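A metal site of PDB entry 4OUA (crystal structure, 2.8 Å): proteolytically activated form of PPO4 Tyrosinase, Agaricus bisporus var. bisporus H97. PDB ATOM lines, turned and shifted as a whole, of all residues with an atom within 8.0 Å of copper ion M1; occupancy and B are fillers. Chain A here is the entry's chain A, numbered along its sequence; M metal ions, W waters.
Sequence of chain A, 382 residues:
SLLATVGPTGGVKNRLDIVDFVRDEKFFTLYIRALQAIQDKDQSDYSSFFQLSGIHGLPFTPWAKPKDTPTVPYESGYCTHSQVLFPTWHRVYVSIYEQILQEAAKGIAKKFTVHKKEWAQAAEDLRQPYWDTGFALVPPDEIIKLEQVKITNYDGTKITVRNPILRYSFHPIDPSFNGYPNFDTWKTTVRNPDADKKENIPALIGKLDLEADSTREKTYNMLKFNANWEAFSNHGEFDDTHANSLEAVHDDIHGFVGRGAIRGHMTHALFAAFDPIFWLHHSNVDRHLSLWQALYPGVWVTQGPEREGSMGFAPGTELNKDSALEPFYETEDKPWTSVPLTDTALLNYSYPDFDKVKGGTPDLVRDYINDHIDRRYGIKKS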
ATOM      1  N   HIS A  56     -28.297   8.205  -8.746  1.00  0.00           N
ATOM      2  CA  HIS A  56     -28.558   6.918  -9.388  1.00  0.00           C
ATOM      3  C   HIS A  56     -28.393   6.995 -10.907  1.00  0.00           C
ATOM      4  O   HIS A  56     -27.533   6.343 -11.485  1.00  0.00           O
ATOM      5  CB  HIS A  56     -29.959   6.420  -9.028  1.00  0.00           C
ATOM      6  CG  HIS A  56     -30.177   4.969  -9.311  1.00  0.00           C
ATOM      7  ND1 HIS A  56     -30.817   4.519 -10.452  1.00  0.00           N
ATOM      8  CD2 HIS A  56     -29.849   3.867  -8.606  1.00  0.00           C
ATOM      9  CE1 HIS A  56     -30.877   3.201 -10.430  1.00  0.00           C
ATOM     10  NE2 HIS A  56     -30.302   2.776  -9.319  1.00  0.00           N
ATOM     11  N   GLY A  57     -29.223   7.813 -11.549  1.00  0.00           N
ATOM     12  CA  GLY A  57     -29.182   7.964 -12.996  1.00  0.00           C
ATOM     13  C   GLY A  57     -28.985   9.408 -13.419  1.00  0.00           C
ATOM     14  O   GLY A  57     -27.982  10.032 -13.057  1.00  0.00           O
ATOM     15  N   TYR A  78     -24.483   6.977 -11.593  1.00  0.00           N
ATOM     16  CA  TYR A  78     -23.510   6.497 -10.613  1.00  0.00           C
ATOM     17  C   TYR A  78     -23.749   5.029 -10.278  1.00  0.00           C
ATOM     18  O   TYR A  78     -22.797   4.293 -10.004  1.00  0.00           O
ATOM     19  CB  TYR A  78     -23.583   7.325  -9.326  1.00  0.00           C
ATOM     20  CG  TYR A  78     -22.628   8.495  -9.269  1.00  0.00           C
ATOM     21  CD1 TYR A  78     -21.250   8.295  -9.281  1.00  0.00           C
ATOM     22  CD2 TYR A  78     -23.091   9.794  -9.169  1.00  0.00           C
ATOM     23  CE1 TYR A  78     -20.374   9.362  -9.215  1.00  0.00           C
ATOM     24  CE2 TYR A  78     -22.227  10.868  -9.107  1.00  0.00           C
ATOM     25  CZ  TYR A  78     -20.861  10.644  -9.128  1.00  0.00           C
ATOM     26  OH  TYR A  78     -19.998  11.708  -9.056  1.00  0.00           O
ATOM     27  N   CYS A  79     -25.010   4.617 -10.299  1.00  0.00           N
ATOM     28  CA  CYS A  79     -25.403   3.289  -9.845  1.00  0.00           C
ATOM     29  C   CYS A  79     -24.681   2.191 -10.615  1.00  0.00           C
ATOM     30  O   CYS A  79     -24.508   2.270 -11.820  1.00  0.00           O
ATOM     31  CB  CYS A  79     -26.922   3.097  -9.955  1.00  0.00           C
ATOM     32  SG  CYS A  79     -27.559   3.023 -11.646  1.00  0.00           S
ATOM     33  N   THR A  80     -24.262   1.166  -9.882  1.00  0.00           N
ATOM     34  CA  THR A  80     -23.553   0.029 -10.462  1.00  0.00           C
ATOM     35  C   THR A  80     -24.512  -1.127 -10.708  1.00  0.00           C
ATOM     36  O   THR A  80     -25.090  -1.672  -9.774  1.00  0.00           O
ATOM     37  CB  THR A  80     -22.402  -0.428  -9.553  1.00  0.00           C
ATOM     38  OG1 THR A  80     -22.946  -0.819  -8.280  1.00  0.00           O
ATOM     39  CG2 THR A  80     -21.401   0.686  -9.347  1.00  0.00           C
ATOM     40  N   HIS A  81     -24.670  -1.488 -11.972  1.00  0.00           N
ATOM     41  CA  HIS A  81     -25.605  -2.539 -12.351  1.00  0.00           C
ATOM     42  C   HIS A  81     -24.938  -3.552 -13.271  1.00  0.00           C
ATOM     43  O   HIS A  81     -24.092  -3.193 -14.086  1.00  0.00           O
ATOM     44  CB  HIS A  81     -26.840  -1.930 -13.032  1.00  0.00           C
ATOM     45  CG  HIS A  81     -27.473  -0.829 -12.233  1.00  0.00           C
ATOM     46  ND1 HIS A  81     -27.370   0.499 -12.587  1.00  0.00           N
ATOM     47  CD2 HIS A  81     -28.218  -0.853 -11.109  1.00  0.00           C
ATOM     48  CE1 HIS A  81     -28.024   1.246 -11.707  1.00  0.00           C
ATOM     49  NE2 HIS A  81     -28.548   0.435 -10.805  1.00  0.00           N
ATOM     50  N   PHE A  86     -22.730  -4.154  -7.326  1.00  0.00           N
ATOM     51  CA  PHE A  86     -24.136  -3.781  -7.189  1.00  0.00           C
ATOM     52  C   PHE A  86     -24.608  -3.734  -5.746  1.00  0.00           C
ATOM     53  O   PHE A  86     -25.142  -2.712  -5.295  1.00  0.00           O
ATOM     54  CB  PHE A  86     -25.020  -4.750  -7.980  1.00  0.00           C
ATOM     55  CG  PHE A  86     -26.493  -4.566  -7.715  1.00  0.00           C
ATOM     56  CD1 PHE A  86     -27.197  -3.539  -8.335  1.00  0.00           C
ATOM     57  CD2 PHE A  86     -27.171  -5.408  -6.853  1.00  0.00           C
ATOM     58  CE1 PHE A  86     -28.543  -3.364  -8.089  1.00  0.00           C
ATOM     59  CE2 PHE A  86     -28.515  -5.243  -6.607  1.00  0.00           C
ATOM     60  CZ  PHE A  86     -29.210  -4.213  -7.223  1.00  0.00           C
ATOM     61  N   TRP A  89     -22.535  -0.944  -3.530  1.00  0.00           N
ATOM     62  CA  TRP A  89     -22.742   0.436  -3.957  1.00  0.00           C
ATOM     63  C   TRP A  89     -24.094   0.957  -3.495  1.00  0.00           C
ATOM     64  O   TRP A  89     -24.236   2.131  -3.137  1.00  0.00           O
ATOM     65  CB  TRP A  89     -22.623   0.584  -5.468  1.00  0.00           C
ATOM     66  CG  TRP A  89     -22.763   2.001  -5.938  1.00  0.00           C
ATOM     67  CD1 TRP A  89     -21.762   2.895  -6.172  1.00  0.00           C
ATOM     68  CD2 TRP A  89     -23.986   2.697  -6.219  1.00  0.00           C
ATOM     69  NE1 TRP A  89     -22.276   4.103  -6.578  1.00  0.00           N
ATOM     70  CE2 TRP A  89     -23.638   4.006  -6.617  1.00  0.00           C
ATOM     71  CE3 TRP A  89     -25.341   2.347  -6.178  1.00  0.00           C
ATOM     72  CZ2 TRP A  89     -24.596   4.954  -6.975  1.00  0.00           C
ATOM     73  CZ3 TRP A  89     -26.288   3.288  -6.531  1.00  0.00           C
ATOM     74  CH2 TRP A  89     -25.915   4.572  -6.920  1.00  0.00           C
ATOM     75  N   HIS A  90     -25.094   0.087  -3.513  1.00  0.00           N
ATOM     76  CA  HIS A  90     -26.445   0.471  -3.141  1.00  0.00           C
ATOM     77  C   HIS A  90     -26.623   0.514  -1.617  1.00  0.00           C
ATOM     78  O   HIS A  90     -27.466   1.252  -1.101  1.00  0.00           O
ATOM     79  CB  HIS A  90     -27.471  -0.468  -3.773  1.00  0.00           C
ATOM     80  CG  HIS A  90     -27.630  -0.277  -5.254  1.00  0.00           C
ATOM     81  ND1 HIS A  90     -26.675  -0.688  -6.165  1.00  0.00           N
ATOM     82  CD2 HIS A  90     -28.609   0.304  -5.974  1.00  0.00           C
ATOM     83  CE1 HIS A  90     -27.075  -0.376  -7.382  1.00  0.00           C
ATOM     84  NE2 HIS A  90     -28.247   0.232  -7.294  1.00  0.00           N
ATOM     85  N   TYR A  93     -25.519   3.743  -0.769  1.00  0.00           N
ATOM     86  CA  TYR A  93     -26.426   4.675  -1.436  1.00  0.00           C
ATOM     87  C   TYR A  93     -27.613   5.015  -0.550  1.00  0.00           C
ATOM     88  O   TYR A  93     -27.990   6.182  -0.411  1.00  0.00           O
ATOM     89  CB  TYR A  93     -26.914   4.102  -2.772  1.00  0.00           C
ATOM     90  CG  TYR A  93     -27.703   5.080  -3.612  1.00  0.00           C
ATOM     91  CD1 TYR A  93     -27.574   6.453  -3.432  1.00  0.00           C
ATOM     92  CD2 TYR A  93     -28.582   4.624  -4.587  1.00  0.00           C
ATOM     93  CE1 TYR A  93     -28.293   7.347  -4.203  1.00  0.00           C
ATOM     94  CE2 TYR A  93     -29.311   5.516  -5.363  1.00  0.00           C
ATOM     95  CZ  TYR A  93     -29.156   6.865  -5.173  1.00  0.00           C
ATOM     96  OH  TYR A  93     -29.877   7.749  -5.936  1.00  0.00           O
ATOM     97  N   GLU A 247     -29.665  -9.006  -7.622  1.00  0.00           N
ATOM     98  CA  GLU A 247     -30.107  -7.951  -8.539  1.00  0.00           C
ATOM     99  C   GLU A 247     -31.228  -8.427  -9.451  1.00  0.00           C
ATOM    100  O   GLU A 247     -32.159  -7.665  -9.735  1.00  0.00           O
ATOM    101  CB  GLU A 247     -28.932  -7.455  -9.379  1.00  0.00           C
ATOM    102  CG  GLU A 247     -29.277  -6.292 -10.297  1.00  0.00           C
ATOM    103  CD  GLU A 247     -28.102  -5.848 -11.153  1.00  0.00           C
ATOM    104  OE1 GLU A 247     -27.131  -6.613 -11.281  1.00  0.00           O
ATOM    105  OE2 GLU A 247     -28.159  -4.723 -11.699  1.00  0.00           O
ATOM    106  N   HIS A 250     -34.186  -8.336  -7.746  1.00  0.00           N
ATOM    107  CA  HIS A 250     -34.395  -6.914  -7.485  1.00  0.00           C
ATOM    108  C   HIS A 250     -35.027  -6.207  -8.685  1.00  0.00           C
ATOM    109  O   HIS A 250     -35.745  -5.220  -8.521  1.00  0.00           O
ATOM    110  CB  HIS A 250     -33.056  -6.265  -7.120  1.00  0.00           C
ATOM    111  CG  HIS A 250     -32.938  -4.842  -7.559  1.00  0.00           C
ATOM    112  ND1 HIS A 250     -32.353  -4.480  -8.760  1.00  0.00           N
ATOM    113  CD2 HIS A 250     -33.313  -3.691  -6.968  1.00  0.00           C
ATOM    114  CE1 HIS A 250     -32.382  -3.168  -8.878  1.00  0.00           C
ATOM    115  NE2 HIS A 250     -32.959  -2.664  -7.808  1.00  0.00           N
ATOM    116  N   ASP A 251     -34.758  -6.712  -9.876  1.00  0.00           N
ATOM    117  CA  ASP A 251     -35.247  -6.093 -11.107  1.00  0.00           C
ATOM    118  C   ASP A 251     -36.759  -6.211 -11.250  1.00  0.00           C
ATOM    119  O   ASP A 251     -37.398  -5.320 -11.809  1.00  0.00           O
ATOM    120  CB  ASP A 251     -34.564  -6.718 -12.327  1.00  0.00           C
ATOM    121  CG  ASP A 251     -33.077  -6.416 -12.378  1.00  0.00           C
ATOM    122  OD1 ASP A 251     -32.657  -5.389 -11.796  1.00  0.00           O
ATOM    123  OD2 ASP A 251     -32.337  -7.195 -13.012  1.00  0.00           O
ATOM    124  N   HIS A 254     -38.852  -3.290  -9.869  1.00  0.00           N
ATOM    125  CA  HIS A 254     -38.816  -2.087 -10.697  1.00  0.00           C
ATOM    126  C   HIS A 254     -39.799  -2.214 -11.857  1.00  0.00           C
ATOM    127  O   HIS A 254     -40.436  -1.245 -12.252  1.00  0.00           O
ATOM    128  CB  HIS A 254     -37.405  -1.809 -11.215  1.00  0.00           C
ATOM    129  CG  HIS A 254     -36.498  -1.210 -10.192  1.00  0.00           C
ATOM    130  ND1 HIS A 254     -36.618   0.086  -9.758  1.00  0.00           N
ATOM    131  CD2 HIS A 254     -35.439  -1.730  -9.530  1.00  0.00           C
ATOM    132  CE1 HIS A 254     -35.679   0.338  -8.862  1.00  0.00           C
ATOM    133  NE2 HIS A 254     -34.945  -0.748  -8.697  1.00  0.00           N
ATOM    134  N   ALA A 269     -33.765   2.884 -15.322  1.00  0.00           N
ATOM    135  CA  ALA A 269     -32.659   3.118 -14.406  1.00  0.00           C
ATOM    136  C   ALA A 269     -32.262   4.589 -14.314  1.00  0.00           C
ATOM    137  O   ALA A 269     -31.640   5.019 -13.338  1.00  0.00           O
ATOM    138  CB  ALA A 269     -31.464   2.279 -14.813  1.00  0.00           C
ATOM    139  N   ALA A 272     -35.535   5.896 -12.106  1.00  0.00           N
ATOM    140  CA  ALA A 272     -36.111   5.056 -11.053  1.00  0.00           C
ATOM    141  C   ALA A 272     -35.919   5.636  -9.655  1.00  0.00           C
ATOM    142  O   ALA A 272     -36.798   5.496  -8.802  1.00  0.00           O
ATOM    143  CB  ALA A 272     -35.511   3.659 -11.121  1.00  0.00           C
ATOM    144  N   ALA A 273     -34.788   6.289  -9.430  1.00  0.00           N
ATOM    145  CA  ALA A 273     -34.460   6.819  -8.117  1.00  0.00           C
ATOM    146  C   ALA A 273     -35.400   7.942  -7.689  1.00  0.00           C
ATOM    147  O   ALA A 273     -35.627   8.159  -6.493  1.00  0.00           O
ATOM    148  CB  ALA A 273     -33.015   7.309  -8.093  1.00  0.00           C
ATOM    149  N   PHE A 278     -38.610   3.967  -4.359  1.00  0.00           N
ATOM    150  CA  PHE A 278     -37.316   3.393  -4.719  1.00  0.00           C
ATOM    151  C   PHE A 278     -36.482   3.069  -3.491  1.00  0.00           C
ATOM    152  O   PHE A 278     -35.731   2.097  -3.474  1.00  0.00           O
ATOM    153  CB  PHE A 278     -36.560   4.356  -5.645  1.00  0.00           C
ATOM    154  CG  PHE A 278     -35.134   3.964  -5.906  1.00  0.00           C
ATOM    155  CD1 PHE A 278     -34.813   3.165  -6.989  1.00  0.00           C
ATOM    156  CD2 PHE A 278     -34.112   4.421  -5.086  1.00  0.00           C
ATOM    157  CE1 PHE A 278     -33.502   2.805  -7.245  1.00  0.00           C
ATOM    158  CE2 PHE A 278     -32.799   4.072  -5.330  1.00  0.00           C
ATOM    159  CZ  PHE A 278     -32.497   3.259  -6.411  1.00  0.00           C
ATOM    160  N   HIS A 282     -34.920  -0.592  -2.034  1.00  0.00           N
ATOM    161  CA  HIS A 282     -33.503  -0.890  -1.861  1.00  0.00           C
ATOM    162  C   HIS A 282     -33.079  -0.930  -0.399  1.00  0.00           C
ATOM    163  O   HIS A 282     -31.960  -1.342  -0.086  1.00  0.00           O
ATOM    164  CB  HIS A 282     -32.667   0.119  -2.646  1.00  0.00           C
ATOM    165  CG  HIS A 282     -32.605  -0.149  -4.110  1.00  0.00           C
ATOM    166  ND1 HIS A 282     -31.569  -0.839  -4.699  1.00  0.00           N
ATOM    167  CD2 HIS A 282     -33.475   0.141  -5.103  1.00  0.00           C
ATOM    168  CE1 HIS A 282     -31.782  -0.936  -5.998  1.00  0.00           C
ATOM    169  NE2 HIS A 282     -32.943  -0.357  -6.272  1.00  0.00           N
HETATM  170 CU    CU M   1     -29.279   1.028  -8.925  1.00  0.00          CU
HETATM  171 CU    CU M   2     -33.015  -0.727  -8.204  1.00  0.00          CU
HETATM  172  O   HOH W   1     -31.379   0.038  -9.581  1.00  0.00           O
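O of His 56 is in hydrogen-bond range of N of Cys 79 (3.3 Å). OH of Tyr 93 is in hydrogen-bond range of N of His 56, 3.3 Å away. A ring nitrogen (ND1) of His 56 lies within hydrogen-bond range of the backbone carbonyl oxygen (O) of Ala 269. N of Tyr 78 sits at hydrogen-bond distance from O of His 56. A ring nitrogen (ND1) of His 90 lies within hydrogen-bond range of the backbone carbonyl oxygen (O) of Phe 86 (2.7 Å). CE1 of His 81 is bonded to SG of Cys 79.
Residues that only touch copper ion M1: Cys 79 (3.3 Å).
Copper ion M1 is bound by a ring nitrogen (NE2) of His 56 (2.1 Å), a ring nitrogen (NE2) of His 90 (2.1 Å), a ring nitrogen (NE2) of His 81 (2.1 Å) and water W1 (2.4 Å).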
